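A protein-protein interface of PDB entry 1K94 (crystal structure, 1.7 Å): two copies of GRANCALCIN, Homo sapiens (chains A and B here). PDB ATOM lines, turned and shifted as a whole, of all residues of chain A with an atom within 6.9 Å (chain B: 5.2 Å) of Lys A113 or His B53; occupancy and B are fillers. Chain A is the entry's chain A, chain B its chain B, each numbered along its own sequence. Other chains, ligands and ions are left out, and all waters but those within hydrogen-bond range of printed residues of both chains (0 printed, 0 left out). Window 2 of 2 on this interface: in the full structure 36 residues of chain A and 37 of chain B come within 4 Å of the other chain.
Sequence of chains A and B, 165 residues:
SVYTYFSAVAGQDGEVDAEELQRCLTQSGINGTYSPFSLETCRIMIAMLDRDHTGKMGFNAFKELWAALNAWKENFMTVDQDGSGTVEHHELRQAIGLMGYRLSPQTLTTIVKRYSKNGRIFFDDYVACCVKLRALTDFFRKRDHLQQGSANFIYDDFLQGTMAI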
ATOM      1  N   LEU A  92      -9.880  23.972   8.293  1.00  0.00           N
ATOM      2  CA  LEU A  92      -9.397  24.814   9.383  1.00  0.00           C
ATOM      3  C   LEU A  92      -8.425  25.846   8.827  1.00  0.00           C
ATOM      4  O   LEU A  92      -8.408  26.996   9.264  1.00  0.00           O
ATOM      5  CB  LEU A  92      -8.697  23.974  10.452  1.00  0.00           C
ATOM      6  CG  LEU A  92      -8.212  24.780  11.664  1.00  0.00           C
ATOM      7  CD1 LEU A  92      -9.409  25.369  12.403  1.00  0.00           C
ATOM      8  CD2 LEU A  92      -7.402  23.883  12.588  1.00  0.00           C
ATOM      9  N   GLN A 106       3.649  24.342   9.273  1.00  0.00           N
ATOM     10  CA  GLN A 106       3.970  23.655  10.516  1.00  0.00           C
ATOM     11  C   GLN A 106       3.070  24.098  11.673  1.00  0.00           C
ATOM     12  O   GLN A 106       2.635  23.270  12.480  1.00  0.00           O
ATOM     13  CB  GLN A 106       5.446  23.869  10.883  1.00  0.00           C
ATOM     14  CG  GLN A 106       5.869  23.118  12.132  1.00  0.00           C
ATOM     15  CD  GLN A 106       7.338  23.287  12.476  1.00  0.00           C
ATOM     16  OE1 GLN A 106       7.859  24.404  12.520  1.00  0.00           O
ATOM     17  NE2 GLN A 106       8.012  22.173  12.739  1.00  0.00           N
ATOM     18  N   LEU A 108       0.099  25.252  11.403  1.00  0.00           N
ATOM     19  CA  LEU A 108      -1.213  24.697  11.094  1.00  0.00           C
ATOM     20  C   LEU A 108      -1.256  23.230  11.512  1.00  0.00           C
ATOM     21  O   LEU A 108      -2.242  22.765  12.081  1.00  0.00           O
ATOM     22  CB  LEU A 108      -1.486  24.823   9.601  1.00  0.00           C
ATOM     23  CG  LEU A 108      -1.541  26.254   9.066  1.00  0.00           C
ATOM     24  CD1 LEU A 108      -1.537  26.221   7.548  1.00  0.00           C
ATOM     25  CD2 LEU A 108      -2.784  26.954   9.601  1.00  0.00           C
ATOM     26  N   THR A 109      -0.179  22.507  11.227  1.00  0.00           N
ATOM     27  CA  THR A 109      -0.075  21.099  11.596  1.00  0.00           C
ATOM     28  C   THR A 109      -0.189  20.962  13.110  1.00  0.00           C
ATOM     29  O   THR A 109      -0.950  20.136  13.621  1.00  0.00           O
ATOM     30  CB  THR A 109       1.276  20.512  11.143  1.00  0.00           C
ATOM     31  OG1 THR A 109       1.235  20.271   9.731  1.00  0.00           O
ATOM     32  CG2 THR A 109       1.579  19.216  11.886  1.00  0.00           C
ATOM     33  N   THR A 110       0.579  21.774  13.824  1.00  0.00           N
ATOM     34  CA  THR A 110       0.562  21.746  15.279  1.00  0.00           C
ATOM     35  C   THR A 110      -0.842  22.004  15.811  1.00  0.00           C
ATOM     36  O   THR A 110      -1.313  21.317  16.717  1.00  0.00           O
ATOM     37  CB  THR A 110       1.530  22.793  15.852  1.00  0.00           C
ATOM     38  OG1 THR A 110       2.873  22.410  15.533  1.00  0.00           O
ATOM     39  CG2 THR A 110       1.374  22.904  17.357  1.00  0.00           C
ATOM     40  N   ILE A 111      -1.519  22.991  15.235  1.00  0.00           N
ATOM     41  CA  ILE A 111      -2.868  23.330  15.671  1.00  0.00           C
ATOM     42  C   ILE A 111      -3.868  22.203  15.438  1.00  0.00           C
ATOM     43  O   ILE A 111      -4.652  21.864  16.325  1.00  0.00           O
ATOM     44  CB  ILE A 111      -3.360  24.610  14.967  1.00  0.00           C
ATOM     45  CG1 ILE A 111      -2.493  25.791  15.414  1.00  0.00           C
ATOM     46  CG2 ILE A 111      -4.833  24.855  15.281  1.00  0.00           C
ATOM     47  CD1 ILE A 111      -2.838  27.113  14.741  1.00  0.00           C
ATOM     48  N   VAL A 112      -3.839  21.612  14.249  1.00  0.00           N
ATOM     49  CA  VAL A 112      -4.760  20.527  13.936  1.00  0.00           C
ATOM     50  C   VAL A 112      -4.572  19.330  14.863  1.00  0.00           C
ATOM     51  O   VAL A 112      -5.547  18.755  15.346  1.00  0.00           O
ATOM     52  CB  VAL A 112      -4.601  20.068  12.464  1.00  0.00           C
ATOM     53  CG1 VAL A 112      -5.382  18.784  12.224  1.00  0.00           C
ATOM     54  CG2 VAL A 112      -5.094  21.162  11.533  1.00  0.00           C
ATOM     55  N   LYS A 113      -3.323  18.958  15.114  1.00  0.00           N
ATOM     56  CA  LYS A 113      -3.023  17.822  15.986  1.00  0.00           C
ATOM     57  C   LYS A 113      -3.442  18.087  17.429  1.00  0.00           C
ATOM     58  O   LYS A 113      -3.941  17.196  18.120  1.00  0.00           O
ATOM     59  CB  LYS A 113      -1.523  17.510  15.946  1.00  0.00           C
ATOM     60  CG  LYS A 113      -1.023  16.962  14.620  1.00  0.00           C
ATOM     61  CD  LYS A 113      -0.949  15.447  14.651  1.00  0.00           C
ATOM     62  CE  LYS A 113      -0.523  14.867  13.307  1.00  0.00           C
ATOM     63  NZ  LYS A 113      -1.612  14.965  12.295  1.00  0.00           N
ATOM     64  N   ARG A 114      -3.242  19.321  17.877  1.00  0.00           N
ATOM     65  CA  ARG A 114      -3.574  19.710  19.239  1.00  0.00           C
ATOM     66  C   ARG A 114      -5.068  19.737  19.533  1.00  0.00           C
ATOM     67  O   ARG A 114      -5.492  19.403  20.639  1.00  0.00           O
ATOM     68  CB  ARG A 114      -2.977  21.090  19.538  1.00  0.00           C
ATOM     69  CG  ARG A 114      -3.329  21.648  20.910  1.00  0.00           C
ATOM     70  CD  ARG A 114      -2.724  20.817  22.034  1.00  0.00           C
ATOM     71  NE  ARG A 114      -3.054  21.377  23.341  1.00  0.00           N
ATOM     72  CZ  ARG A 114      -4.274  21.378  23.867  1.00  0.00           C
ATOM     73  NH1 ARG A 114      -5.287  20.835  23.197  1.00  0.00           N
ATOM     74  NH2 ARG A 114      -4.489  21.932  25.054  1.00  0.00           N
ATOM     75  N   TYR A 115      -5.864  20.118  18.537  1.00  0.00           N
ATOM     76  CA  TYR A 115      -7.306  20.229  18.711  1.00  0.00           C
ATOM     77  C   TYR A 115      -8.153  19.079  18.182  1.00  0.00           C
ATOM     78  O   TYR A 115      -9.373  19.094  18.327  1.00  0.00           O
ATOM     79  CB  TYR A 115      -7.779  21.551  18.099  1.00  0.00           C
ATOM     80  CG  TYR A 115      -7.375  22.751  18.924  1.00  0.00           C
ATOM     81  CD1 TYR A 115      -8.174  23.189  19.981  1.00  0.00           C
ATOM     82  CD2 TYR A 115      -6.167  23.408  18.692  1.00  0.00           C
ATOM     83  CE1 TYR A 115      -7.776  24.253  20.791  1.00  0.00           C
ATOM     84  CE2 TYR A 115      -5.760  24.472  19.498  1.00  0.00           C
ATOM     85  CZ  TYR A 115      -6.569  24.887  20.545  1.00  0.00           C
ATOM     86  OH  TYR A 115      -6.168  25.932  21.345  1.00  0.00           O
ATOM     87  N   SER A 116      -7.516  18.085  17.576  1.00  0.00           N
ATOM     88  CA  SER A 116      -8.260  16.949  17.048  1.00  0.00           C
ATOM     89  C   SER A 116      -8.565  15.930  18.137  1.00  0.00           C
ATOM     90  O   SER A 116      -7.756  15.706  19.038  1.00  0.00           O
ATOM     91  CB  SER A 116      -7.474  16.258  15.926  1.00  0.00           C
ATOM     92  OG  SER A 116      -7.395  17.073  14.772  1.00  0.00           O
ATOM     93  N   LYS A 117      -9.748  15.332  18.048  1.00  0.00           N
ATOM     94  CA  LYS A 117     -10.186  14.298  18.981  1.00  0.00           C
ATOM     95  C   LYS A 117     -10.611  13.108  18.138  1.00  0.00           C
ATOM     96  O   LYS A 117     -11.575  13.194  17.380  1.00  0.00           O
ATOM     97  CB  LYS A 117     -11.376  14.770  19.822  1.00  0.00           C
ATOM     98  CG  LYS A 117     -11.001  15.637  21.009  1.00  0.00           C
ATOM     99  CD  LYS A 117     -12.208  15.900  21.898  1.00  0.00           C
ATOM    100  CE  LYS A 117     -11.803  16.600  23.179  1.00  0.00           C
ATOM    101  NZ  LYS A 117     -12.985  16.827  24.047  1.00  0.00           N
ATOM    102  N   ILE A 121     -11.858  17.719  14.416  1.00  0.00           N
ATOM    103  CA  ILE A 121     -12.001  18.919  15.231  1.00  0.00           C
ATOM    104  C   ILE A 121     -13.471  19.301  15.278  1.00  0.00           C
ATOM    105  O   ILE A 121     -14.031  19.795  14.296  1.00  0.00           O
ATOM    106  CB  ILE A 121     -11.196  20.100  14.654  1.00  0.00           C
ATOM    107  CG1 ILE A 121      -9.720  19.714  14.536  1.00  0.00           C
ATOM    108  CG2 ILE A 121     -11.337  21.319  15.563  1.00  0.00           C
ATOM    109  CD1 ILE A 121      -8.839  20.813  13.967  1.00  0.00           C
ATOM    110  N   ASP B  50       5.518  15.915  22.513  1.00  0.00           N
ATOM    111  CA  ASP B  50       5.223  15.545  21.131  1.00  0.00           C
ATOM    112  C   ASP B  50       6.239  16.165  20.170  1.00  0.00           C
ATOM    113  O   ASP B  50       5.879  16.947  19.289  1.00  0.00           O
ATOM    114  CB  ASP B  50       3.799  15.990  20.788  1.00  0.00           C
ATOM    115  CG  ASP B  50       3.279  15.370  19.507  1.00  0.00           C
ATOM    116  OD1 ASP B  50       3.826  14.332  19.079  1.00  0.00           O
ATOM    117  OD2 ASP B  50       2.312  15.915  18.935  1.00  0.00           O
ATOM    118  N   ARG B  51       7.505  15.799  20.346  1.00  0.00           N
ATOM    119  CA  ARG B  51       8.593  16.327  19.523  1.00  0.00           C
ATOM    120  C   ARG B  51       8.456  16.026  18.032  1.00  0.00           C
ATOM    121  O   ARG B  51       9.015  16.741  17.201  1.00  0.00           O
ATOM    122  CB  ARG B  51       9.947  15.806  20.025  1.00  0.00           C
ATOM    123  CG  ARG B  51      10.245  16.137  21.488  1.00  0.00           C
ATOM    124  CD  ARG B  51      11.727  15.962  21.814  1.00  0.00           C
ATOM    125  NE  ARG B  51      12.050  16.351  23.186  1.00  0.00           N
ATOM    126  CZ  ARG B  51      11.972  15.544  24.239  1.00  0.00           C
ATOM    127  NH1 ARG B  51      11.580  14.287  24.085  1.00  0.00           N
ATOM    128  NH2 ARG B  51      12.289  15.992  25.447  1.00  0.00           N
ATOM    129  N   ASP B  52       7.719  14.973  17.691  1.00  0.00           N
ATOM    130  CA  ASP B  52       7.526  14.615  16.290  1.00  0.00           C
ATOM    131  C   ASP B  52       6.123  14.974  15.793  1.00  0.00           C
ATOM    132  O   ASP B  52       5.667  14.482  14.759  1.00  0.00           O
ATOM    133  CB  ASP B  52       7.812  13.122  16.085  1.00  0.00           C
ATOM    134  CG  ASP B  52       6.987  12.238  16.999  1.00  0.00           C
ATOM    135  OD1 ASP B  52       6.394  12.768  17.962  1.00  0.00           O
ATOM    136  OD2 ASP B  52       6.940  11.010  16.764  1.00  0.00           O
ATOM    137  N   HIS B  53       5.454  15.839  16.552  1.00  0.00           N
ATOM    138  CA  HIS B  53       4.113  16.336  16.236  1.00  0.00           C
ATOM    139  C   HIS B  53       3.132  15.323  15.645  1.00  0.00           C
ATOM    140  O   HIS B  53       2.595  15.536  14.556  1.00  0.00           O
ATOM    141  CB  HIS B  53       4.233  17.532  15.287  1.00  0.00           C
ATOM    142  CG  HIS B  53       5.280  18.519  15.693  1.00  0.00           C
ATOM    143  ND1 HIS B  53       5.153  19.331  16.800  1.00  0.00           N
ATOM    144  CD2 HIS B  53       6.495  18.794  15.164  1.00  0.00           C
ATOM    145  CE1 HIS B  53       6.244  20.064  16.933  1.00  0.00           C
ATOM    146  NE2 HIS B  53       7.074  19.756  15.953  1.00  0.00           N
ATOM    147  N   THR B  54       2.885  14.235  16.368  1.00  0.00           N
ATOM    148  CA  THR B  54       1.955  13.208  15.907  1.00  0.00           C
ATOM    149  C   THR B  54       0.688  13.229  16.753  1.00  0.00           C
ATOM    150  O   THR B  54      -0.256  12.481  16.496  1.00  0.00           O
ATOM    151  CB  THR B  54       2.569  11.804  16.013  1.00  0.00           C
ATOM    152  OG1 THR B  54       2.801  11.488  17.393  1.00  0.00           O
ATOM    153  CG2 THR B  54       3.884  11.742  15.253  1.00  0.00           C
ATOM    154  N   GLY B  55       0.674  14.089  17.766  1.00  0.00           N
ATOM    155  CA  GLY B  55      -0.481  14.176  18.637  1.00  0.00           C
ATOM    156  C   GLY B  55      -0.603  12.934  19.498  1.00  0.00           C
ATOM    157  O   GLY B  55      -1.634  12.702  20.120  1.00  0.00           O
ATOM    158  N   GLN B 160       2.977  29.027  17.208  1.00  0.00           N
ATOM    159  CA  GLN B 160       3.154  27.582  17.183  1.00  0.00           C
ATOM    160  C   GLN B 160       3.523  27.043  18.559  1.00  0.00           C
ATOM    161  O   GLN B 160       2.955  26.049  19.015  1.00  0.00           O
ATOM    162  CB  GLN B 160       4.223  27.166  16.172  1.00  0.00           C
ATOM    163  CG  GLN B 160       4.602  25.700  16.316  1.00  0.00           C
ATOM    164  CD  GLN B 160       5.498  25.203  15.210  1.00  0.00           C
ATOM    165  OE1 GLN B 160       6.441  25.882  14.802  1.00  0.00           O
ATOM    166  NE2 GLN B 160       5.220  23.997  14.728  1.00  0.00           N
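O of Gln A106 lies within hydrogen-bond range of OG1 of Thr A110 (3.2 Å).
The side-chain carboxylate of Asp B50 lies within hydrogen-bond range of the backbone NH of His B53.
The side-chain carboxylate (OD1) of Asp B50 lies within hydrogen-bond range of the backbone NH (N) of Thr B54 (2.9 Å).
The backbone NH (N) of Gly B55 sits at hydrogen-bond distance from the side-chain carboxylate (OD2) of Asp B50, at 2.7 Å.
Of chain A, only Lys A113 comes within 4 Å of His B53.
Printed residues of chain B within 4 Å of Gln A106: Gln B160 (2.8 Å).
Printed residues of chain A within 4 Å of Gly B55: Lys A113 (3.8 Å).
Printed residues of chain A within 4 Å of Gln B160: Gln A106 (2.8 Å) and Thr A110 (2.9 Å).
Of the printed residues of chain A, Thr B54 touches Lys A113 (3.5 Å).
Of the printed residues of chain B, Thr A110 touches Gln B160.
Asp B50 touches none of the printed residues of chain A.
Ser A116 touches none of the printed residues of chain B.
The nearest residue of chain A that does not touch His B53 is Thr A110 (4.04 Å).
The nearest printed residue of chain B that does not touch Thr A110 is His B53 (4.04 Å).
Of the 13 printed residues of chain A, 3 touch a printed residue of chain B.
Printed residues of chain A that touch a printed residue of chain B: Gln A106, Thr A110 and Lys A113.
Of the 7 printed residues of chain B, 4 touch a printed residue of chain A.
The side-chain amide oxygen (OE1) of Gln A106 sits close to the side-chain amide oxygen (OE1) of Gln B160.
The side-chain amide nitrogen (NE2) of Gln B160 sits at hydrogen-bond distance from the side-chain hydroxyl (OG1) of Thr A110, at 2.9 Å.
No position is printed for both chains.
Among the printed residues, pairs that only touch across the chains: Lys A113 with His B53 (3.4 Å), Lys A113 with Thr B54 (3.5 Å) and Lys A113 with Gly B55 (3.8 Å).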
